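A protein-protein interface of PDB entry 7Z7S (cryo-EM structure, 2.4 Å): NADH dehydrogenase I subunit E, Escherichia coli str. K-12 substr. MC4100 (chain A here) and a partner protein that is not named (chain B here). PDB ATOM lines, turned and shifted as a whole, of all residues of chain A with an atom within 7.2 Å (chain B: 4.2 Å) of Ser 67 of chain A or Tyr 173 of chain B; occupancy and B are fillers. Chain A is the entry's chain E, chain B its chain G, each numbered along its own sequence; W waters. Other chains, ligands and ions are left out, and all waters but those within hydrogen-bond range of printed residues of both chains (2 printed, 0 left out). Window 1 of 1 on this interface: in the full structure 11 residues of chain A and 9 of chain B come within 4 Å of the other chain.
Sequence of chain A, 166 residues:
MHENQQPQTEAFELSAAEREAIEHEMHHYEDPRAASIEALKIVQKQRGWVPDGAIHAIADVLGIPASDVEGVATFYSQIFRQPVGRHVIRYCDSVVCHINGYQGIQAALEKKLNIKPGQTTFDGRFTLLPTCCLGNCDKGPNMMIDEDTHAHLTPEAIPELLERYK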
ATOM      1  N   ILE A  55      21.648  33.504 -19.459  1.00  0.00           N
ATOM      2  CA  ILE A  55      22.903  33.226 -20.154  1.00  0.00           C
ATOM      3  C   ILE A  55      23.100  34.205 -21.302  1.00  0.00           C
ATOM      4  O   ILE A  55      24.157  34.835 -21.435  1.00  0.00           O
ATOM      5  CB  ILE A  55      22.928  31.768 -20.647  1.00  0.00           C
ATOM      6  CG1 ILE A  55      22.802  30.800 -19.471  1.00  0.00           C
ATOM      7  CG2 ILE A  55      24.190  31.490 -21.442  1.00  0.00           C
ATOM      8  CD1 ILE A  55      23.906  30.928 -18.454  1.00  0.00           C
ATOM      9  N   HIS A  56      22.057  34.393 -22.112  1.00  0.00           N
ATOM     10  CA  HIS A  56      22.152  35.303 -23.246  1.00  0.00           C
ATOM     11  C   HIS A  56      22.206  36.754 -22.792  1.00  0.00           C
ATOM     12  O   HIS A  56      22.916  37.565 -23.394  1.00  0.00           O
ATOM     13  CB  HIS A  56      20.980  35.076 -24.197  1.00  0.00           C
ATOM     14  CG  HIS A  56      21.303  34.170 -25.343  1.00  0.00           C
ATOM     15  ND1 HIS A  56      21.676  34.642 -26.582  1.00  0.00           N
ATOM     16  CD2 HIS A  56      21.309  32.820 -25.436  1.00  0.00           C
ATOM     17  CE1 HIS A  56      21.899  33.621 -27.390  1.00  0.00           C
ATOM     18  NE2 HIS A  56      21.682  32.504 -26.719  1.00  0.00           N
ATOM     19  N   ALA A  59      25.738  37.322 -21.479  1.00  0.00           N
ATOM     20  CA  ALA A  59      26.637  37.335 -22.626  1.00  0.00           C
ATOM     21  C   ALA A  59      26.533  38.638 -23.406  1.00  0.00           C
ATOM     22  O   ALA A  59      27.543  39.167 -23.880  1.00  0.00           O
ATOM     23  CB  ALA A  59      26.329  36.148 -23.532  1.00  0.00           C
ATOM     24  N   ILE A  64      30.696  38.714 -24.669  1.00  0.00           N
ATOM     25  CA  ILE A  64      31.313  37.420 -24.940  1.00  0.00           C
ATOM     26  C   ILE A  64      30.207  36.496 -25.438  1.00  0.00           C
ATOM     27  O   ILE A  64      29.027  36.805 -25.234  1.00  0.00           O
ATOM     28  CB  ILE A  64      32.034  36.872 -23.694  1.00  0.00           C
ATOM     29  CG1 ILE A  64      31.040  36.512 -22.592  1.00  0.00           C
ATOM     30  CG2 ILE A  64      33.044  37.879 -23.185  1.00  0.00           C
ATOM     31  CD1 ILE A  64      31.694  35.992 -21.340  1.00  0.00           C
ATOM     32  N   PRO A  65      30.520  35.404 -26.138  1.00  0.00           N
ATOM     33  CA  PRO A  65      29.461  34.508 -26.617  1.00  0.00           C
ATOM     34  C   PRO A  65      28.698  33.829 -25.491  1.00  0.00           C
ATOM     35  O   PRO A  65      29.209  33.627 -24.389  1.00  0.00           O
ATOM     36  CB  PRO A  65      30.225  33.476 -27.453  1.00  0.00           C
ATOM     37  CG  PRO A  65      31.437  34.164 -27.874  1.00  0.00           C
ATOM     38  CD  PRO A  65      31.810  35.098 -26.776  1.00  0.00           C
ATOM     39  N   ALA A  66      27.445  33.474 -25.796  1.00  0.00           N
ATOM     40  CA  ALA A  66      26.619  32.746 -24.841  1.00  0.00           C
ATOM     41  C   ALA A  66      27.162  31.353 -24.568  1.00  0.00           C
ATOM     42  O   ALA A  66      26.919  30.802 -23.491  1.00  0.00           O
ATOM     43  CB  ALA A  66      25.180  32.661 -25.342  1.00  0.00           C
ATOM     44  N   SER A  67      27.890  30.772 -25.523  1.00  0.00           N
ATOM     45  CA  SER A  67      28.500  29.470 -25.295  1.00  0.00           C
ATOM     46  C   SER A  67      29.559  29.538 -24.201  1.00  0.00           C
ATOM     47  O   SER A  67      29.661  28.623 -23.379  1.00  0.00           O
ATOM     48  CB  SER A  67      29.084  28.922 -26.598  1.00  0.00           C
ATOM     49  OG  SER A  67      29.913  29.869 -27.242  1.00  0.00           O
ATOM     50  N   ASP A  68      30.338  30.624 -24.155  1.00  0.00           N
ATOM     51  CA  ASP A  68      31.305  30.793 -23.072  1.00  0.00           C
ATOM     52  C   ASP A  68      30.621  30.967 -21.722  1.00  0.00           C
ATOM     53  O   ASP A  68      31.063  30.385 -20.723  1.00  0.00           O
ATOM     54  CB  ASP A  68      32.235  31.974 -23.350  1.00  0.00           C
ATOM     55  CG  ASP A  68      33.100  31.759 -24.567  1.00  0.00           C
ATOM     56  OD1 ASP A  68      33.538  30.613 -24.792  1.00  0.00           O
ATOM     57  OD2 ASP A  68      33.376  32.735 -25.284  1.00  0.00           O
ATOM     58  N   VAL A  69      29.545  31.754 -21.675  1.00  0.00           N
ATOM     59  CA  VAL A  69      28.808  31.959 -20.431  1.00  0.00           C
ATOM     60  C   VAL A  69      28.209  30.650 -19.938  1.00  0.00           C
ATOM     61  O   VAL A  69      28.274  30.333 -18.746  1.00  0.00           O
ATOM     62  CB  VAL A  69      27.730  33.043 -20.617  1.00  0.00           C
ATOM     63  CG1 VAL A  69      26.882  33.179 -19.365  1.00  0.00           C
ATOM     64  CG2 VAL A  69      28.376  34.366 -20.953  1.00  0.00           C
ATOM     65  N   GLU A  70      27.636  29.859 -20.844  1.00  0.00           N
ATOM     66  CA  GLU A  70      27.048  28.592 -20.429  1.00  0.00           C
ATOM     67  C   GLU A  70      28.113  27.573 -20.041  1.00  0.00           C
ATOM     68  O   GLU A  70      27.897  26.785 -19.114  1.00  0.00           O
ATOM     69  CB  GLU A  70      26.127  28.049 -21.526  1.00  0.00           C
ATOM     70  CG  GLU A  70      25.499  26.690 -21.221  1.00  0.00           C
ATOM     71  CD  GLU A  70      24.284  26.761 -20.298  1.00  0.00           C
ATOM     72  OE1 GLU A  70      24.383  27.324 -19.193  1.00  0.00           O
ATOM     73  OE2 GLU A  70      23.224  26.221 -20.670  1.00  0.00           O
ATOM     74  N   GLY A  71      29.270  27.587 -20.707  1.00  0.00           N
ATOM     75  CA  GLY A  71      30.367  26.733 -20.283  1.00  0.00           C
ATOM     76  C   GLY A  71      30.863  27.072 -18.892  1.00  0.00           C
ATOM     77  O   GLY A  71      31.173  26.180 -18.099  1.00  0.00           O
ATOM     78  N   VAL A  72      30.915  28.363 -18.569  1.00  0.00           N
ATOM     79  CA  VAL A  72      31.256  28.777 -17.213  1.00  0.00           C
ATOM     80  C   VAL A  72      30.174  28.338 -16.229  1.00  0.00           C
ATOM     81  O   VAL A  72      30.472  27.760 -15.181  1.00  0.00           O
ATOM     82  CB  VAL A  72      31.493  30.296 -17.164  1.00  0.00           C
ATOM     83  CG1 VAL A  72      31.581  30.776 -15.738  1.00  0.00           C
ATOM     84  CG2 VAL A  72      32.757  30.654 -17.919  1.00  0.00           C
ATOM     85  N   ALA A  73      28.905  28.574 -16.569  1.00  0.00           N
ATOM     86  CA  ALA A  73      27.811  28.299 -15.639  1.00  0.00           C
ATOM     87  C   ALA A  73      27.697  26.814 -15.327  1.00  0.00           C
ATOM     88  O   ALA A  73      27.451  26.434 -14.178  1.00  0.00           O
ATOM     89  CB  ALA A  73      26.495  28.828 -16.203  1.00  0.00           C
ATOM     90  N   THR A  74      27.893  25.959 -16.325  1.00  0.00           N
ATOM     91  CA  THR A  74      27.848  24.522 -16.113  1.00  0.00           C
ATOM     92  C   THR A  74      29.172  23.940 -15.639  1.00  0.00           C
ATOM     93  O   THR A  74      29.199  22.777 -15.232  1.00  0.00           O
ATOM     94  CB  THR A  74      27.413  23.806 -17.393  1.00  0.00           C
ATOM     95  OG1 THR A  74      28.328  24.118 -18.445  1.00  0.00           O
ATOM     96  CG2 THR A  74      26.026  24.239 -17.799  1.00  0.00           C
ATOM     97  N   PHE A  75      30.270  24.699 -15.694  1.00  0.00           N
ATOM     98  CA  PHE A  75      31.508  24.220 -15.087  1.00  0.00           C
ATOM     99  C   PHE A  75      31.437  24.280 -13.567  1.00  0.00           C
ATOM    100  O   PHE A  75      31.794  23.317 -12.883  1.00  0.00           O
ATOM    101  CB  PHE A  75      32.704  25.030 -15.590  1.00  0.00           C
ATOM    102  CG  PHE A  75      34.028  24.524 -15.090  1.00  0.00           C
ATOM    103  CD1 PHE A  75      34.664  23.475 -15.725  1.00  0.00           C
ATOM    104  CD2 PHE A  75      34.631  25.091 -13.982  1.00  0.00           C
ATOM    105  CE1 PHE A  75      35.873  23.002 -15.268  1.00  0.00           C
ATOM    106  CE2 PHE A  75      35.834  24.619 -13.518  1.00  0.00           C
ATOM    107  CZ  PHE A  75      36.460  23.577 -14.164  1.00  0.00           C
ATOM    108  N   LYS B 162      36.006  27.616 -32.373  1.00  0.00           N
ATOM    109  CA  LYS B 162      36.136  28.868 -31.658  1.00  0.00           C
ATOM    110  C   LYS B 162      37.469  29.552 -31.935  1.00  0.00           C
ATOM    111  O   LYS B 162      37.485  30.734 -32.280  1.00  0.00           O
ATOM    112  CB  LYS B 162      35.952  28.622 -30.160  1.00  0.00           C
ATOM    113  CG  LYS B 162      35.676  29.865 -29.359  1.00  0.00           C
ATOM    114  CD  LYS B 162      35.257  29.528 -27.945  1.00  0.00           C
ATOM    115  CE  LYS B 162      33.856  28.983 -27.908  1.00  0.00           C
ATOM    116  NZ  LYS B 162      33.505  28.454 -26.569  1.00  0.00           N
ATOM    117  N   THR B 168      31.048  31.303 -32.657  1.00  0.00           N
ATOM    118  CA  THR B 168      30.628  31.672 -31.316  1.00  0.00           C
ATOM    119  C   THR B 168      29.618  30.730 -30.682  1.00  0.00           C
ATOM    120  O   THR B 168      29.425  30.803 -29.466  1.00  0.00           O
ATOM    121  CB  THR B 168      30.027  33.086 -31.308  1.00  0.00           C
ATOM    122  OG1 THR B 168      28.856  33.116 -32.129  1.00  0.00           O
ATOM    123  CG2 THR B 168      31.025  34.098 -31.834  1.00  0.00           C
ATOM    124  N   LEU B 170      29.420  27.248 -30.638  1.00  0.00           N
ATOM    125  CA  LEU B 170      29.824  25.933 -30.160  1.00  0.00           C
ATOM    126  C   LEU B 170      30.727  26.102 -28.952  1.00  0.00           C
ATOM    127  O   LEU B 170      31.511  27.047 -28.887  1.00  0.00           O
ATOM    128  CB  LEU B 170      30.540  25.127 -31.247  1.00  0.00           C
ATOM    129  CG  LEU B 170      30.635  23.614 -31.053  1.00  0.00           C
ATOM    130  CD1 LEU B 170      29.405  22.935 -31.606  1.00  0.00           C
ATOM    131  CD2 LEU B 170      31.877  23.063 -31.717  1.00  0.00           C
ATOM    132  N   GLY B 171      30.609  25.192 -27.995  1.00  0.00           N
ATOM    133  CA  GLY B 171      31.386  25.288 -26.776  1.00  0.00           C
ATOM    134  C   GLY B 171      31.370  23.981 -26.015  1.00  0.00           C
ATOM    135  O   GLY B 171      30.746  22.996 -26.423  1.00  0.00           O
ATOM    136  N   VAL B 172      32.084  23.988 -24.896  1.00  0.00           N
ATOM    137  CA  VAL B 172      32.164  22.847 -23.997  1.00  0.00           C
ATOM    138  C   VAL B 172      31.480  23.229 -22.692  1.00  0.00           C
ATOM    139  O   VAL B 172      31.680  24.332 -22.174  1.00  0.00           O
ATOM    140  CB  VAL B 172      33.622  22.393 -23.784  1.00  0.00           C
ATOM    141  CG1 VAL B 172      34.524  23.558 -23.421  1.00  0.00           C
ATOM    142  CG2 VAL B 172      33.713  21.271 -22.764  1.00  0.00           C
ATOM    143  N   TYR B 173      30.632  22.339 -22.195  1.00  0.00           N
ATOM    144  CA  TYR B 173      29.823  22.563 -21.011  1.00  0.00           C
ATOM    145  C   TYR B 173      30.016  21.413 -20.044  1.00  0.00           C
ATOM    146  O   TYR B 173      30.529  20.352 -20.393  1.00  0.00           O
ATOM    147  CB  TYR B 173      28.344  22.720 -21.375  1.00  0.00           C
ATOM    148  CG  TYR B 173      28.170  23.516 -22.626  1.00  0.00           C
ATOM    149  CD1 TYR B 173      28.372  24.888 -22.623  1.00  0.00           C
ATOM    150  CD2 TYR B 173      27.859  22.899 -23.822  1.00  0.00           C
ATOM    151  CE1 TYR B 173      28.244  25.621 -23.769  1.00  0.00           C
ATOM    152  CE2 TYR B 173      27.730  23.625 -24.972  1.00  0.00           C
ATOM    153  CZ  TYR B 173      27.922  24.983 -24.940  1.00  0.00           C
ATOM    154  OH  TYR B 173      27.795  25.704 -26.091  1.00  0.00           O
ATOM    155  N   GLY B 174      29.602  21.643 -18.815  1.00  0.00           N
ATOM    156  CA  GLY B 174      29.722  20.635 -17.801  1.00  0.00           C
ATOM    157  C   GLY B 174      31.138  20.525 -17.274  1.00  0.00           C
ATOM    158  O   GLY B 174      31.967  21.417 -17.407  1.00  0.00           O
ATOM    159  N   ALA B 175      31.411  19.369 -16.693  1.00  0.00           N
ATOM    160  CA  ALA B 175      32.601  19.139 -15.899  1.00  0.00           C
ATOM    161  C   ALA B 175      32.984  17.679 -16.067  1.00  0.00           C
ATOM    162  O   ALA B 175      32.577  17.028 -17.033  1.00  0.00           O
ATOM    163  CB  ALA B 175      32.376  19.550 -14.435  1.00  0.00           C
ATOM    164  N   ASN B 178      31.404  14.382 -17.418  1.00  0.00           N
ATOM    165  CA  ASN B 178      30.163  14.790 -18.048  1.00  0.00           C
ATOM    166  C   ASN B 178      30.357  15.994 -18.961  1.00  0.00           C
ATOM    167  O   ASN B 178      29.432  16.784 -19.146  1.00  0.00           O
ATOM    168  CB  ASN B 178      29.119  15.096 -16.978  1.00  0.00           C
ATOM    169  CG  ASN B 178      27.727  14.721 -17.403  1.00  0.00           C
ATOM    170  OD1 ASN B 178      27.519  13.704 -18.055  1.00  0.00           O
ATOM    171  ND2 ASN B 178      26.762  15.547 -17.045  1.00  0.00           N
ATOM    172  N   VAL B 179      31.557  16.162 -19.521  1.00  0.00           N
ATOM    173  CA  VAL B 179      31.799  17.268 -20.441  1.00  0.00           C
ATOM    174  C   VAL B 179      31.007  17.045 -21.721  1.00  0.00           C
ATOM    175  O   VAL B 179      30.979  15.942 -22.278  1.00  0.00           O
ATOM    176  CB  VAL B 179      33.299  17.440 -20.731  1.00  0.00           C
ATOM    177  CG1 VAL B 179      33.950  18.302 -19.666  1.00  0.00           C
ATOM    178  CG2 VAL B 179      33.996  16.102 -20.849  1.00  0.00           C
ATOM    179  N   TYR B 180      30.348  18.096 -22.178  1.00  0.00           N
ATOM    180  CA  TYR B 180      29.454  18.076 -23.318  1.00  0.00           C
ATOM    181  C   TYR B 180      29.963  19.067 -24.350  1.00  0.00           C
ATOM    182  O   TYR B 180      30.359  20.177 -24.007  1.00  0.00           O
ATOM    183  CB  TYR B 180      28.045  18.443 -22.876  1.00  0.00           C
ATOM    184  CG  TYR B 180      26.945  18.078 -23.829  1.00  0.00           C
ATOM    185  CD1 TYR B 180      26.557  18.951 -24.834  1.00  0.00           C
ATOM    186  CD2 TYR B 180      26.273  16.875 -23.709  1.00  0.00           C
ATOM    187  CE1 TYR B 180      25.543  18.632 -25.696  1.00  0.00           C
ATOM    188  CE2 TYR B 180      25.254  16.545 -24.570  1.00  0.00           C
ATOM    189  CZ  TYR B 180      24.895  17.428 -25.563  1.00  0.00           C
ATOM    190  OH  TYR B 180      23.882  17.106 -26.426  1.00  0.00           O
ATOM    191  N   GLY B 182      28.927  21.069 -27.792  1.00  0.00           N
ATOM    192  CA  GLY B 182      27.796  21.392 -28.638  1.00  0.00           C
ATOM    193  C   GLY B 182      27.401  22.845 -28.498  1.00  0.00           C
ATOM    194  O   GLY B 182      28.197  23.677 -28.079  1.00  0.00           O
ATOM    195  N   ARG B 183      26.185  23.126 -28.863  1.00  0.00           N
ATOM    196  CA  ARG B 183      25.635  24.466 -28.773  1.00  0.00           C
ATOM    197  C   ARG B 183      24.981  24.682 -27.416  1.00  0.00           C
ATOM    198  O   ARG B 183      24.634  23.719 -26.731  1.00  0.00           O
ATOM    199  CB  ARG B 183      24.627  24.682 -29.893  1.00  0.00           C
ATOM    200  CG  ARG B 183      25.208  24.589 -31.274  1.00  0.00           C
ATOM    201  CD  ARG B 183      24.199  25.001 -32.317  1.00  0.00           C
ATOM    202  NE  ARG B 183      24.173  26.436 -32.570  1.00  0.00           N
ATOM    203  CZ  ARG B 183      23.204  27.249 -32.174  1.00  0.00           C
ATOM    204  NH1 ARG B 183      22.181  26.807 -31.465  1.00  0.00           N
ATOM    205  NH2 ARG B 183      23.263  28.534 -32.498  1.00  0.00           N
ATOM    206  N   PRO B 184      24.817  25.936 -26.973  1.00  0.00           N
ATOM    207  CA  PRO B 184      24.088  26.165 -25.715  1.00  0.00           C
ATOM    208  C   PRO B 184      22.625  25.760 -25.774  1.00  0.00           C
ATOM    209  O   PRO B 184      22.022  25.532 -24.721  1.00  0.00           O
ATOM    210  CB  PRO B 184      24.251  27.671 -25.481  1.00  0.00           C
ATOM    211  CG  PRO B 184      24.555  28.233 -26.801  1.00  0.00           C
ATOM    212  CD  PRO B 184      25.337  27.200 -27.527  1.00  0.00           C
HETATM  213  O   HOH W   1      26.845  31.218 -28.452  1.00  0.00           O
HETATM  214  O   HOH W   2      32.190  26.600 -23.181  1.00  0.00           O
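The backbone carbonyl oxygen of Gly 182 of chain B sits at hydrogen-bond distance from the side-chain hydroxyl of Tyr 173 of chain B, at 2.9 Å. The backbone NH (N) of Tyr 173 of chain B is in hydrogen-bond range of the backbone carbonyl oxygen (O) of Tyr 180 of chain B, 2.8 Å away. The backbone carbonyl oxygen of Leu 170 of chain B lies close to the side-chain amino group of Lys 162 of chain B. N of Gly 171 of chain B sits at hydrogen-bond distance from OH of Tyr 173 of chain B, 3.4 Å away. The backbone carbonyl oxygen (O) of Glu 70 of chain A lies within hydrogen-bond range of the side-chain hydroxyl (OG1) of Thr 74 of chain A.
Water W2 lies within hydrogen-bond range of O of Val 172 of chain B (2.5 Å) and O of Ser 67 of chain A (3.2 Å). Water W1 lies within hydrogen-bond range of the backbone carbonyl oxygen (O) of Thr 168 of chain B and the backbone NH (N) of Ser 67 of chain A.
Among the printed residues, merely in contact across the chains: Pro 65 of chain A with Thr 168 of chain B (3.4 Å), Ser 67 of chain A with Lys 162 of chain B (3.9 Å), Ser 67 of chain A with Leu 170 of chain B (3.6 Å), Ser 67 of chain A with Tyr 173 of chain B (3.3 Å), Glu 70 of chain A with Tyr 173 of chain B (3.7 Å), Gly 71 of chain A with Val 172 of chain B (3.3 Å), Gly 71 of chain A with Tyr 173 of chain B (3.4 Å), Thr 74 of chain A with Tyr 173 of chain B (3.2 Å) and Phe 75 of chain A with Gly 174 of chain B (3.7 Å).
NZ of Lys 162 of chain B is in salt-bridge range of OD1 of Asp 68 of chain A (2.8 Å). The backbone carbonyl oxygen of Thr 168 of chain B is in hydrogen-bond range of the side-chain hydroxyl of Ser 67 of chain A (2.5 Å). The side-chain hydroxyl (OG1) of Thr 74 of chain A lies within hydrogen-bond range of the backbone NH (N) of Gly 174 of chain B.
Of the 15 printed residues of chain A, 7 touch a printed residue of chain B. Hydrophobic or aromatic side chains of chain A that line the printed part of chain B: Pro 65 and Phe 75. Among the printed residues, Asp or Glu carboxylates within 4 Å of a Lys or Arg side-chain nitrogen of the other chain: Asp 68 of chain A with Lys 162 of chain B (2.8 Å).
Of the printed residues of chain B, Pro 65 of chain A touches Thr 168 (3.4 Å). Ser 67 of chain A touches just these residues of chain B: Lys 162, Thr 168, Leu 170 and Tyr 173. Printed residues of chain B within 4 Å of Glu 70 of chain A: Tyr 173. Tyr 173 of chain B touches just these residues of chain A: Ser 67, Glu 70, Gly 71 and Thr 74. The nearest printed residue of chain B that does not touch Ser 67 of chain A is Pro 184 of chain B (4.2 Å). The nearest residue of chain A that does not touch Tyr 173 of chain B is Ala 66 of chain A (5.4 Å). The nearest printed residue of chain A that does not touch Lys 162 of chain B is Pro 65 of chain A (5.7 Å).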
